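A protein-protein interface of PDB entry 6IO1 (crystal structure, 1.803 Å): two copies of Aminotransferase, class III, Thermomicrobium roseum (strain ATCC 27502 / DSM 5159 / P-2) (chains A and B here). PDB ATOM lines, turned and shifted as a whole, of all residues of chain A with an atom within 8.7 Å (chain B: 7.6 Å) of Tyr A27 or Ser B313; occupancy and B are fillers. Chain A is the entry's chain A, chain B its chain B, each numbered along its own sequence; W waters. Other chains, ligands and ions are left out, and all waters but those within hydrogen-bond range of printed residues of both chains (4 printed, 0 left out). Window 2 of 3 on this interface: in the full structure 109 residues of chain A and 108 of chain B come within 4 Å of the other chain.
The backbone NH (N) of Phe B318 lies within hydrogen-bond range of the backbone carbonyl oxygen (O) of Thr A24, 2.9 Å away. ND2 of Asn A25 sits at hydrogen-bond distance from OD1 of Asp B315 (3.0 Å). N of Arg B316 sits close to ND2 of Asn A25 (3.4 Å). OE1 of Glu B309 is in salt-bridge range of NH1 of Arg A30 (2.9 Å).
The side-chain amide oxygen (OD1) of Asn A25 sits at hydrogen-bond distance from the backbone NH (N) of Tyr A27. OD1 of Asn A25 lies within hydrogen-bond range of N of Gln A28 (2.8 Å). O of Tyr A27 sits at hydrogen-bond distance from NH1 of Arg A31, 3.0 Å away. The side-chain hydroxyl of Ser B313 lies within hydrogen-bond range of the backbone carbonyl oxygen of Thr B310 (2.8 Å).
Val B317 touches Thr A24 (CA to O, 3.8 Å). Asn A25 touches Ala B314 (OD1 to O, 3.99 Å). CA of Val B317 touches CA of Asn A25, 3.97 Å away. CA of Ala B312 touches CB of Leu A26 (3.8 Å). Tyr A27 touches Ala B312. Ser B313 touches Tyr A27 (O to CD2, 3.9 Å). CB of Tyr A27 touches O of Ala B314 (3.3 Å). Tyr A27 touches Asp B315 (CD1 to OD1, 3.7 Å). Arg A30 touches Ala B308 (NH2 to O, 3.8 Å). Ala B312 touches Arg A30.
Printed residues of chain B within 4 Å of Tyr A27: Ala B312, Ser B313, Ala B314 and Asp B315. Ser B313 touches one residue of chain A. Of chain A, only Leu A26 (3.8 Å), Tyr A27 (3.4 Å) and Arg A30 (3.4 Å) come within 4 Å of Ala B312. Printed residues of chain B within 4 Å of Asn A25: Ala B314, Asp B315, Arg B316 and Val B317. Of the printed residues of chain A, Asp B315 touches Asn A25 and Tyr A27. Ile A16 touches none of the printed residues of chain B. The nearest residue of chain A that does not touch Ser B313 is Leu A26 (6.0 Å).
Printed residues of chain A that touch a printed residue of chain B: Thr A24, Asn A25, Leu A26, Tyr A27 and Arg A30. Of the 14 printed residues of chain B, 10 touch a printed residue of chain A. Printed residues of chain B that touch a printed residue of chain A: Ala B308, Glu B309, Leu B311, Ala B312, Ser B313, Ala B314, Asp B315, Arg B316, Val B317 and Phe B318. Among the printed residues, Asp or Glu carboxylates within 4 Å of a Lys or Arg side-chain nitrogen of the other chain: Arg A30 with Glu B309 (2.9 Å).
No position is printed for both chains.
Water W1 lies within hydrogen-bond range of the backbone carbonyl oxygen of Arg B316 (2.5 Å), the backbone carbonyl oxygen of Ala B314 (3.1 Å) and the backbone NH of Leu A26 (3.1 Å). Water W4 lies within hydrogen-bond range of O of Ala B312 and NH1 of Arg A31. Water W2 bridges NH2 of Arg A30 (2.7 Å) and OE1 of Glu B309 (2.9 Å). Water W3 bridges NH1 of Arg A30 and OE2 of Glu B309.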
ATOM      1  N   ILE A  16      18.235  10.071 -13.615  1.00  0.00           N
ATOM      2  CA  ILE A  16      18.562   9.988 -15.035  1.00  0.00           C
ATOM      3  C   ILE A  16      18.296   8.582 -15.558  1.00  0.00           C
ATOM      4  O   ILE A  16      17.813   8.402 -16.684  1.00  0.00           O
ATOM      5  CB  ILE A  16      20.022  10.419 -15.276  1.00  0.00           C
ATOM      6  CG1 ILE A  16      20.187  11.913 -14.991  1.00  0.00           C
ATOM      7  CG2 ILE A  16      20.451  10.108 -16.702  1.00  0.00           C
ATOM      8  CD1 ILE A  16      21.627  12.371 -14.954  1.00  0.00           C
ATOM      9  N   LEU A  20      11.193   9.170 -16.071  1.00  0.00           N
ATOM     10  CA  LEU A  20      10.712   9.800 -17.302  1.00  0.00           C
ATOM     11  C   LEU A  20       9.913  11.040 -16.911  1.00  0.00           C
ATOM     12  O   LEU A  20       8.693  10.997 -16.755  1.00  0.00           O
ATOM     13  CB  LEU A  20       9.877   8.818 -18.115  1.00  0.00           C
ATOM     14  CG  LEU A  20       9.530   9.211 -19.551  1.00  0.00           C
ATOM     15  CD1 LEU A  20      10.709   8.951 -20.476  1.00  0.00           C
ATOM     16  CD2 LEU A  20       8.297   8.459 -20.028  1.00  0.00           C
ATOM     17  N   THR A  24       9.407  18.028 -19.419  1.00  0.00           N
ATOM     18  CA  THR A  24      10.846  18.189 -19.284  1.00  0.00           C
ATOM     19  C   THR A  24      11.517  17.830 -20.600  1.00  0.00           C
ATOM     20  O   THR A  24      11.045  16.961 -21.338  1.00  0.00           O
ATOM     21  CB  THR A  24      11.394  17.305 -18.146  1.00  0.00           C
ATOM     22  OG1 THR A  24      10.776  17.679 -16.909  1.00  0.00           O
ATOM     23  CG2 THR A  24      12.906  17.441 -18.008  1.00  0.00           C
ATOM     24  N   ASN A  25      12.622  18.512 -20.892  1.00  0.00           N
ATOM     25  CA  ASN A  25      13.466  18.151 -22.025  1.00  0.00           C
ATOM     26  C   ASN A  25      14.298  16.955 -21.582  1.00  0.00           C
ATOM     27  O   ASN A  25      15.302  17.105 -20.882  1.00  0.00           O
ATOM     28  CB  ASN A  25      14.338  19.329 -22.448  1.00  0.00           C
ATOM     29  CG  ASN A  25      15.141  19.051 -23.710  1.00  0.00           C
ATOM     30  OD1 ASN A  25      15.654  17.951 -23.913  1.00  0.00           O
ATOM     31  ND2 ASN A  25      15.255  20.058 -24.566  1.00  0.00           N
ATOM     32  N   LEU A  26      13.868  15.756 -21.984  1.00  0.00           N
ATOM     33  CA  LEU A  26      14.546  14.538 -21.550  1.00  0.00           C
ATOM     34  C   LEU A  26      15.980  14.502 -22.060  1.00  0.00           C
ATOM     35  O   LEU A  26      16.889  14.032 -21.360  1.00  0.00           O
ATOM     36  CB  LEU A  26      13.761  13.317 -22.030  1.00  0.00           C
ATOM     37  CG  LEU A  26      12.288  13.304 -21.607  1.00  0.00           C
ATOM     38  CD1 LEU A  26      11.531  12.160 -22.266  1.00  0.00           C
ATOM     39  CD2 LEU A  26      12.165  13.229 -20.093  1.00  0.00           C
ATOM     40  N   TYR A  27      16.200  15.010 -23.275  1.00  0.00           N
ATOM     41  CA  TYR A  27      17.547  15.100 -23.828  1.00  0.00           C
ATOM     42  C   TYR A  27      18.436  15.953 -22.933  1.00  0.00           C
ATOM     43  O   TYR A  27      19.570  15.574 -22.617  1.00  0.00           O
ATOM     44  CB  TYR A  27      17.471  15.675 -25.245  1.00  0.00           C
ATOM     45  CG  TYR A  27      18.792  15.903 -25.951  1.00  0.00           C
ATOM     46  CD1 TYR A  27      19.568  17.027 -25.683  1.00  0.00           C
ATOM     47  CD2 TYR A  27      19.246  15.013 -26.916  1.00  0.00           C
ATOM     48  CE1 TYR A  27      20.766  17.241 -26.334  1.00  0.00           C
ATOM     49  CE2 TYR A  27      20.441  15.222 -27.575  1.00  0.00           C
ATOM     50  CZ  TYR A  27      21.198  16.336 -27.280  1.00  0.00           C
ATOM     51  OH  TYR A  27      22.390  16.546 -27.933  1.00  0.00           O
ATOM     52  N   GLN A  28      17.932  17.116 -22.513  1.00  0.00           N
ATOM     53  CA  GLN A  28      18.680  17.957 -21.585  1.00  0.00           C
ATOM     54  C   GLN A  28      18.828  17.291 -20.224  1.00  0.00           C
ATOM     55  O   GLN A  28      19.875  17.413 -19.580  1.00  0.00           O
ATOM     56  CB  GLN A  28      18.000  19.320 -21.441  1.00  0.00           C
ATOM     57  CG  GLN A  28      18.575  20.178 -20.325  1.00  0.00           C
ATOM     58  CD  GLN A  28      17.913  21.537 -20.228  1.00  0.00           C
ATOM     59  OE1 GLN A  28      17.036  21.870 -21.024  1.00  0.00           O
ATOM     60  NE2 GLN A  28      18.331  22.330 -19.248  1.00  0.00           N
ATOM     61  N   LEU A  29      17.780  16.604 -19.757  1.00  0.00           N
ATOM     62  CA  LEU A  29      17.828  15.983 -18.437  1.00  0.00           C
ATOM     63  C   LEU A  29      18.933  14.940 -18.349  1.00  0.00           C
ATOM     64  O   LEU A  29      19.640  14.858 -17.338  1.00  0.00           O
ATOM     65  CB  LEU A  29      16.479  15.351 -18.099  1.00  0.00           C
ATOM     66  CG  LEU A  29      16.475  14.563 -16.786  1.00  0.00           C
ATOM     67  CD1 LEU A  29      16.062  15.451 -15.619  1.00  0.00           C
ATOM     68  CD2 LEU A  29      15.581  13.340 -16.893  1.00  0.00           C
ATOM     69  N   ARG A  30      19.094  14.126 -19.395  1.00  0.00           N
ATOM     70  CA  ARG A  30      20.127  13.093 -19.356  1.00  0.00           C
ATOM     71  C   ARG A  30      21.523  13.703 -19.256  1.00  0.00           C
ATOM     72  O   ARG A  30      22.409  13.139 -18.605  1.00  0.00           O
ATOM     73  CB  ARG A  30      20.011  12.187 -20.582  1.00  0.00           C
ATOM     74  CG  ARG A  30      18.747  11.344 -20.569  1.00  0.00           C
ATOM     75  CD  ARG A  30      18.842  10.126 -21.471  1.00  0.00           C
ATOM     76  NE  ARG A  30      17.787   9.164 -21.156  1.00  0.00           N
ATOM     77  CZ  ARG A  30      17.663   7.968 -21.723  1.00  0.00           C
ATOM     78  NH1 ARG A  30      18.516   7.582 -22.660  1.00  0.00           N
ATOM     79  NH2 ARG A  30      16.670   7.165 -21.363  1.00  0.00           N
ATOM     80  N   ARG A  31      21.737  14.853 -19.898  1.00  0.00           N
ATOM     81  CA  ARG A  31      23.050  15.492 -19.874  1.00  0.00           C
ATOM     82  C   ARG A  31      23.300  16.278 -18.589  1.00  0.00           C
ATOM     83  O   ARG A  31      24.420  16.270 -18.067  1.00  0.00           O
ATOM     84  CB  ARG A  31      23.210  16.389 -21.102  1.00  0.00           C
ATOM     85  CG  ARG A  31      23.484  15.593 -22.363  1.00  0.00           C
ATOM     86  CD  ARG A  31      22.839  16.194 -23.595  1.00  0.00           C
ATOM     87  NE  ARG A  31      23.069  15.347 -24.763  1.00  0.00           N
ATOM     88  CZ  ARG A  31      22.373  14.248 -25.040  1.00  0.00           C
ATOM     89  NH1 ARG A  31      21.385  13.866 -24.241  1.00  0.00           N
ATOM     90  NH2 ARG A  31      22.657  13.536 -26.121  1.00  0.00           N
ATOM     91  N   GLU A  32      22.283  16.967 -18.067  1.00  0.00           N
ATOM     92  CA  GLU A  32      22.466  17.862 -16.933  1.00  0.00           C
ATOM     93  C   GLU A  32      21.908  17.334 -15.619  1.00  0.00           C
ATOM     94  O   GLU A  32      22.359  17.777 -14.558  1.00  0.00           O
ATOM     95  CB  GLU A  32      21.827  19.231 -17.221  1.00  0.00           C
ATOM     96  CG  GLU A  32      22.293  19.868 -18.520  1.00  0.00           C
ATOM     97  CD  GLU A  32      21.597  21.184 -18.808  1.00  0.00           C
ATOM     98  OE1 GLU A  32      20.785  21.624 -17.967  1.00  0.00           O
ATOM     99  OE2 GLU A  32      21.862  21.776 -19.874  1.00  0.00           O
ATOM    100  N   GLY A  33      20.949  16.415 -15.655  1.00  0.00           N
ATOM    101  CA  GLY A  33      20.370  15.886 -14.444  1.00  0.00           C
ATOM    102  C   GLY A  33      19.263  16.763 -13.900  1.00  0.00           C
ATOM    103  O   GLY A  33      19.017  17.872 -14.387  1.00  0.00           O
ATOM    104  N   LYS A 399      17.144  29.757 -27.065  1.00  0.00           N
ATOM    105  CA  LYS A 399      16.876  28.969 -25.861  1.00  0.00           C
ATOM    106  C   LYS A 399      16.661  29.875 -24.650  1.00  0.00           C
ATOM    107  O   LYS A 399      17.301  29.722 -23.607  1.00  0.00           O
ATOM    108  CB  LYS A 399      17.998  27.961 -25.598  1.00  0.00           C
ATOM    109  CG  LYS A 399      18.149  26.889 -26.666  1.00  0.00           C
ATOM    110  CD  LYS A 399      19.283  25.931 -26.325  1.00  0.00           C
ATOM    111  CE  LYS A 399      19.348  24.773 -27.308  1.00  0.00           C
ATOM    112  NZ  LYS A 399      20.505  23.877 -27.033  1.00  0.00           N
ATOM    113  N   LEU B 138       8.054  10.149 -33.291  1.00  0.00           N
ATOM    114  CA  LEU B 138       9.488  10.420 -33.285  1.00  0.00           C
ATOM    115  C   LEU B 138      10.234   9.523 -34.263  1.00  0.00           C
ATOM    116  O   LEU B 138      11.299   9.901 -34.764  1.00  0.00           O
ATOM    117  CB  LEU B 138      10.047  10.243 -31.874  1.00  0.00           C
ATOM    118  CG  LEU B 138       9.706  11.333 -30.856  1.00  0.00           C
ATOM    119  CD1 LEU B 138      10.153  10.916 -29.465  1.00  0.00           C
ATOM    120  CD2 LEU B 138      10.343  12.656 -31.248  1.00  0.00           C
ATOM    121  N   LYS B 139       9.698   8.337 -34.543  1.00  0.00           N
ATOM    122  CA  LYS B 139      10.321   7.404 -35.471  1.00  0.00           C
ATOM    123  C   LYS B 139      10.018   7.727 -36.927  1.00  0.00           C
ATOM    124  O   LYS B 139      10.445   6.978 -37.812  1.00  0.00           O
ATOM    125  CB  LYS B 139       9.869   5.975 -35.162  1.00  0.00           C
ATOM    126  CG  LYS B 139      10.367   5.428 -33.834  1.00  0.00           C
ATOM    127  CD  LYS B 139      11.867   5.202 -33.851  1.00  0.00           C
ATOM    128  CE  LYS B 139      12.273   4.166 -32.815  1.00  0.00           C
ATOM    129  NZ  LYS B 139      13.735   4.196 -32.540  1.00  0.00           N
ATOM    130  N   ILE B 307      12.022   2.508 -25.866  1.00  0.00           N
ATOM    131  CA  ILE B 307      11.060   3.605 -25.945  1.00  0.00           C
ATOM    132  C   ILE B 307      11.610   4.845 -25.251  1.00  0.00           C
ATOM    133  O   ILE B 307      11.508   5.967 -25.765  1.00  0.00           O
ATOM    134  CB  ILE B 307       9.707   3.175 -25.348  1.00  0.00           C
ATOM    135  CG1 ILE B 307       9.032   2.145 -26.255  1.00  0.00           C
ATOM    136  CG2 ILE B 307       8.804   4.380 -25.132  1.00  0.00           C
ATOM    137  CD1 ILE B 307       7.732   1.610 -25.705  1.00  0.00           C
ATOM    138  N   ALA B 308      12.191   4.660 -24.065  1.00  0.00           N
ATOM    139  CA  ALA B 308      12.754   5.786 -23.329  1.00  0.00           C
ATOM    140  C   ALA B 308      13.908   6.425 -24.089  1.00  0.00           C
ATOM    141  O   ALA B 308      14.049   7.652 -24.095  1.00  0.00           O
ATOM    142  CB  ALA B 308      13.212   5.333 -21.947  1.00  0.00           C
ATOM    143  N   GLU B 309      14.761   5.610 -24.711  1.00  0.00           N
ATOM    144  CA  GLU B 309      15.863   6.148 -25.501  1.00  0.00           C
ATOM    145  C   GLU B 309      15.342   6.957 -26.681  1.00  0.00           C
ATOM    146  O   GLU B 309      15.861   8.040 -26.982  1.00  0.00           O
ATOM    147  CB  GLU B 309      16.759   5.007 -25.985  1.00  0.00           C
ATOM    148  CG  GLU B 309      18.041   5.455 -26.662  1.00  0.00           C
ATOM    149  CD  GLU B 309      19.123   5.821 -25.669  1.00  0.00           C
ATOM    150  OE1 GLU B 309      19.040   5.375 -24.504  1.00  0.00           O
ATOM    151  OE2 GLU B 309      20.059   6.552 -26.053  1.00  0.00           O
ATOM    152  N   THR B 310      14.302   6.452 -27.349  1.00  0.00           N
ATOM    153  CA  THR B 310      13.699   7.194 -28.451  1.00  0.00           C
ATOM    154  C   THR B 310      13.148   8.531 -27.969  1.00  0.00           C
ATOM    155  O   THR B 310      13.368   9.572 -28.600  1.00  0.00           O
ATOM    156  CB  THR B 310      12.597   6.361 -29.107  1.00  0.00           C
ATOM    157  OG1 THR B 310      13.170   5.191 -29.704  1.00  0.00           O
ATOM    158  CG2 THR B 310      11.882   7.171 -30.180  1.00  0.00           C
ATOM    159  N   LEU B 311      12.428   8.519 -26.843  1.00  0.00           N
ATOM    160  CA  LEU B 311      11.876   9.758 -26.304  1.00  0.00           C
ATOM    161  C   LEU B 311      12.978  10.741 -25.926  1.00  0.00           C
ATOM    162  O   LEU B 311      12.875  11.941 -26.208  1.00  0.00           O
ATOM    163  CB  LEU B 311      10.992   9.462 -25.091  1.00  0.00           C
ATOM    164  CG  LEU B 311       9.716   8.632 -25.267  1.00  0.00           C
ATOM    165  CD1 LEU B 311       8.666   9.061 -24.252  1.00  0.00           C
ATOM    166  CD2 LEU B 311       9.163   8.731 -26.682  1.00  0.00           C
ATOM    167  N   ALA B 312      14.042  10.254 -25.286  1.00  0.00           N
ATOM    168  CA  ALA B 312      15.131  11.105 -24.827  1.00  0.00           C
ATOM    169  C   ALA B 312      16.090  11.505 -25.939  1.00  0.00           C
ATOM    170  O   ALA B 312      16.999  12.305 -25.689  1.00  0.00           O
ATOM    171  CB  ALA B 312      15.907  10.405 -23.709  1.00  0.00           C
ATOM    172  N   SER B 313      15.917  10.978 -27.151  1.00  0.00           N
ATOM    173  CA  SER B 313      16.779  11.371 -28.258  1.00  0.00           C
ATOM    174  C   SER B 313      16.368  12.694 -28.891  1.00  0.00           C
ATOM    175  O   SER B 313      17.133  13.240 -29.695  1.00  0.00           O
ATOM    176  CB  SER B 313      16.796  10.275 -29.327  1.00  0.00           C
ATOM    177  OG  SER B 313      15.609  10.302 -30.102  1.00  0.00           O
ATOM    178  N   ALA B 314      15.192  13.222 -28.555  1.00  0.00           N
ATOM    179  CA  ALA B 314      14.710  14.471 -29.127  1.00  0.00           C
ATOM    180  C   ALA B 314      15.069  15.639 -28.216  1.00  0.00           C
ATOM    181  O   ALA B 314      14.730  15.636 -27.027  1.00  0.00           O
ATOM    182  CB  ALA B 314      13.198  14.415 -29.345  1.00  0.00           C
ATOM    183  N   ASP B 315      15.747  16.640 -28.780  1.00  0.00           N
ATOM    184  CA  ASP B 315      16.121  17.846 -28.040  1.00  0.00           C
ATOM    185  C   ASP B 315      14.931  18.807 -28.028  1.00  0.00           C
ATOM    186  O   ASP B 315      14.904  19.844 -28.694  1.00  0.00           O
ATOM    187  CB  ASP B 315      17.360  18.487 -28.650  1.00  0.00           C
ATOM    188  CG  ASP B 315      17.874  19.659 -27.834  1.00  0.00           C
ATOM    189  OD1 ASP B 315      17.395  19.856 -26.696  1.00  0.00           O
ATOM    190  OD2 ASP B 315      18.762  20.385 -28.331  1.00  0.00           O
ATOM    191  N   ARG B 316      13.928  18.433 -27.239  1.00  0.00           N
ATOM    192  CA  ARG B 316      12.701  19.205 -27.116  1.00  0.00           C
ATOM    193  C   ARG B 316      12.039  18.840 -25.798  1.00  0.00           C
ATOM    194  O   ARG B 316      12.370  17.826 -25.178  1.00  0.00           O
ATOM    195  CB  ARG B 316      11.750  18.938 -28.285  1.00  0.00           C
ATOM    196  CG  ARG B 316      11.141  17.547 -28.253  1.00  0.00           C
ATOM    197  CD  ARG B 316      10.577  17.140 -29.605  1.00  0.00           C
ATOM    198  NE  ARG B 316       9.393  17.914 -29.971  1.00  0.00           N
ATOM    199  CZ  ARG B 316       8.199  17.774 -29.404  1.00  0.00           C
ATOM    200  NH1 ARG B 316       7.182  18.524 -29.808  1.00  0.00           N
ATOM    201  NH2 ARG B 316       8.015  16.887 -28.434  1.00  0.00           N
ATOM    202  N   VAL B 317      11.103  19.679 -25.374  1.00  0.00           N
ATOM    203  CA  VAL B 317      10.355  19.415 -24.152  1.00  0.00           C
ATOM    204  C   VAL B 317       9.291  18.366 -24.436  1.00  0.00           C
ATOM    205  O   VAL B 317       8.588  18.429 -25.452  1.00  0.00           O
ATOM    206  CB  VAL B 317       9.729  20.712 -23.609  1.00  0.00           C
ATOM    207  CG1 VAL B 317       8.871  20.420 -22.386  1.00  0.00           C
ATOM    208  CG2 VAL B 317      10.810  21.728 -23.278  1.00  0.00           C
ATOM    209  N   PHE B 318       9.171  17.391 -23.539  1.00  0.00           N
ATOM    210  CA  PHE B 318       8.116  16.388 -23.635  1.00  0.00           C
ATOM    211  C   PHE B 318       6.830  17.022 -23.122  1.00  0.00           C
ATOM    212  O   PHE B 318       6.651  17.189 -21.911  1.00  0.00           O
ATOM    213  CB  PHE B 318       8.495  15.144 -22.834  1.00  0.00           C
ATOM    214  CG  PHE B 318       7.469  14.048 -22.882  1.00  0.00           C
ATOM    215  CD1 PHE B 318       6.953  13.616 -24.091  1.00  0.00           C
ATOM    216  CD2 PHE B 318       7.033  13.440 -21.717  1.00  0.00           C
ATOM    217  CE1 PHE B 318       6.013  12.603 -24.137  1.00  0.00           C
ATOM    218  CE2 PHE B 318       6.093  12.426 -21.756  1.00  0.00           C
ATOM    219  CZ  PHE B 318       5.583  12.007 -22.968  1.00  0.00           C
HETATM  220  O   HOH W   1      12.638  15.399 -24.812  1.00  0.00           O
HETATM  221  O   HOH W   2      17.115   4.689 -22.453  1.00  0.00           O
HETATM  222  O   HOH W   3      20.597   8.836 -24.070  1.00  0.00           O
HETATM  223  O   HOH W   4      19.520  11.688 -25.211  1.00  0.00           O
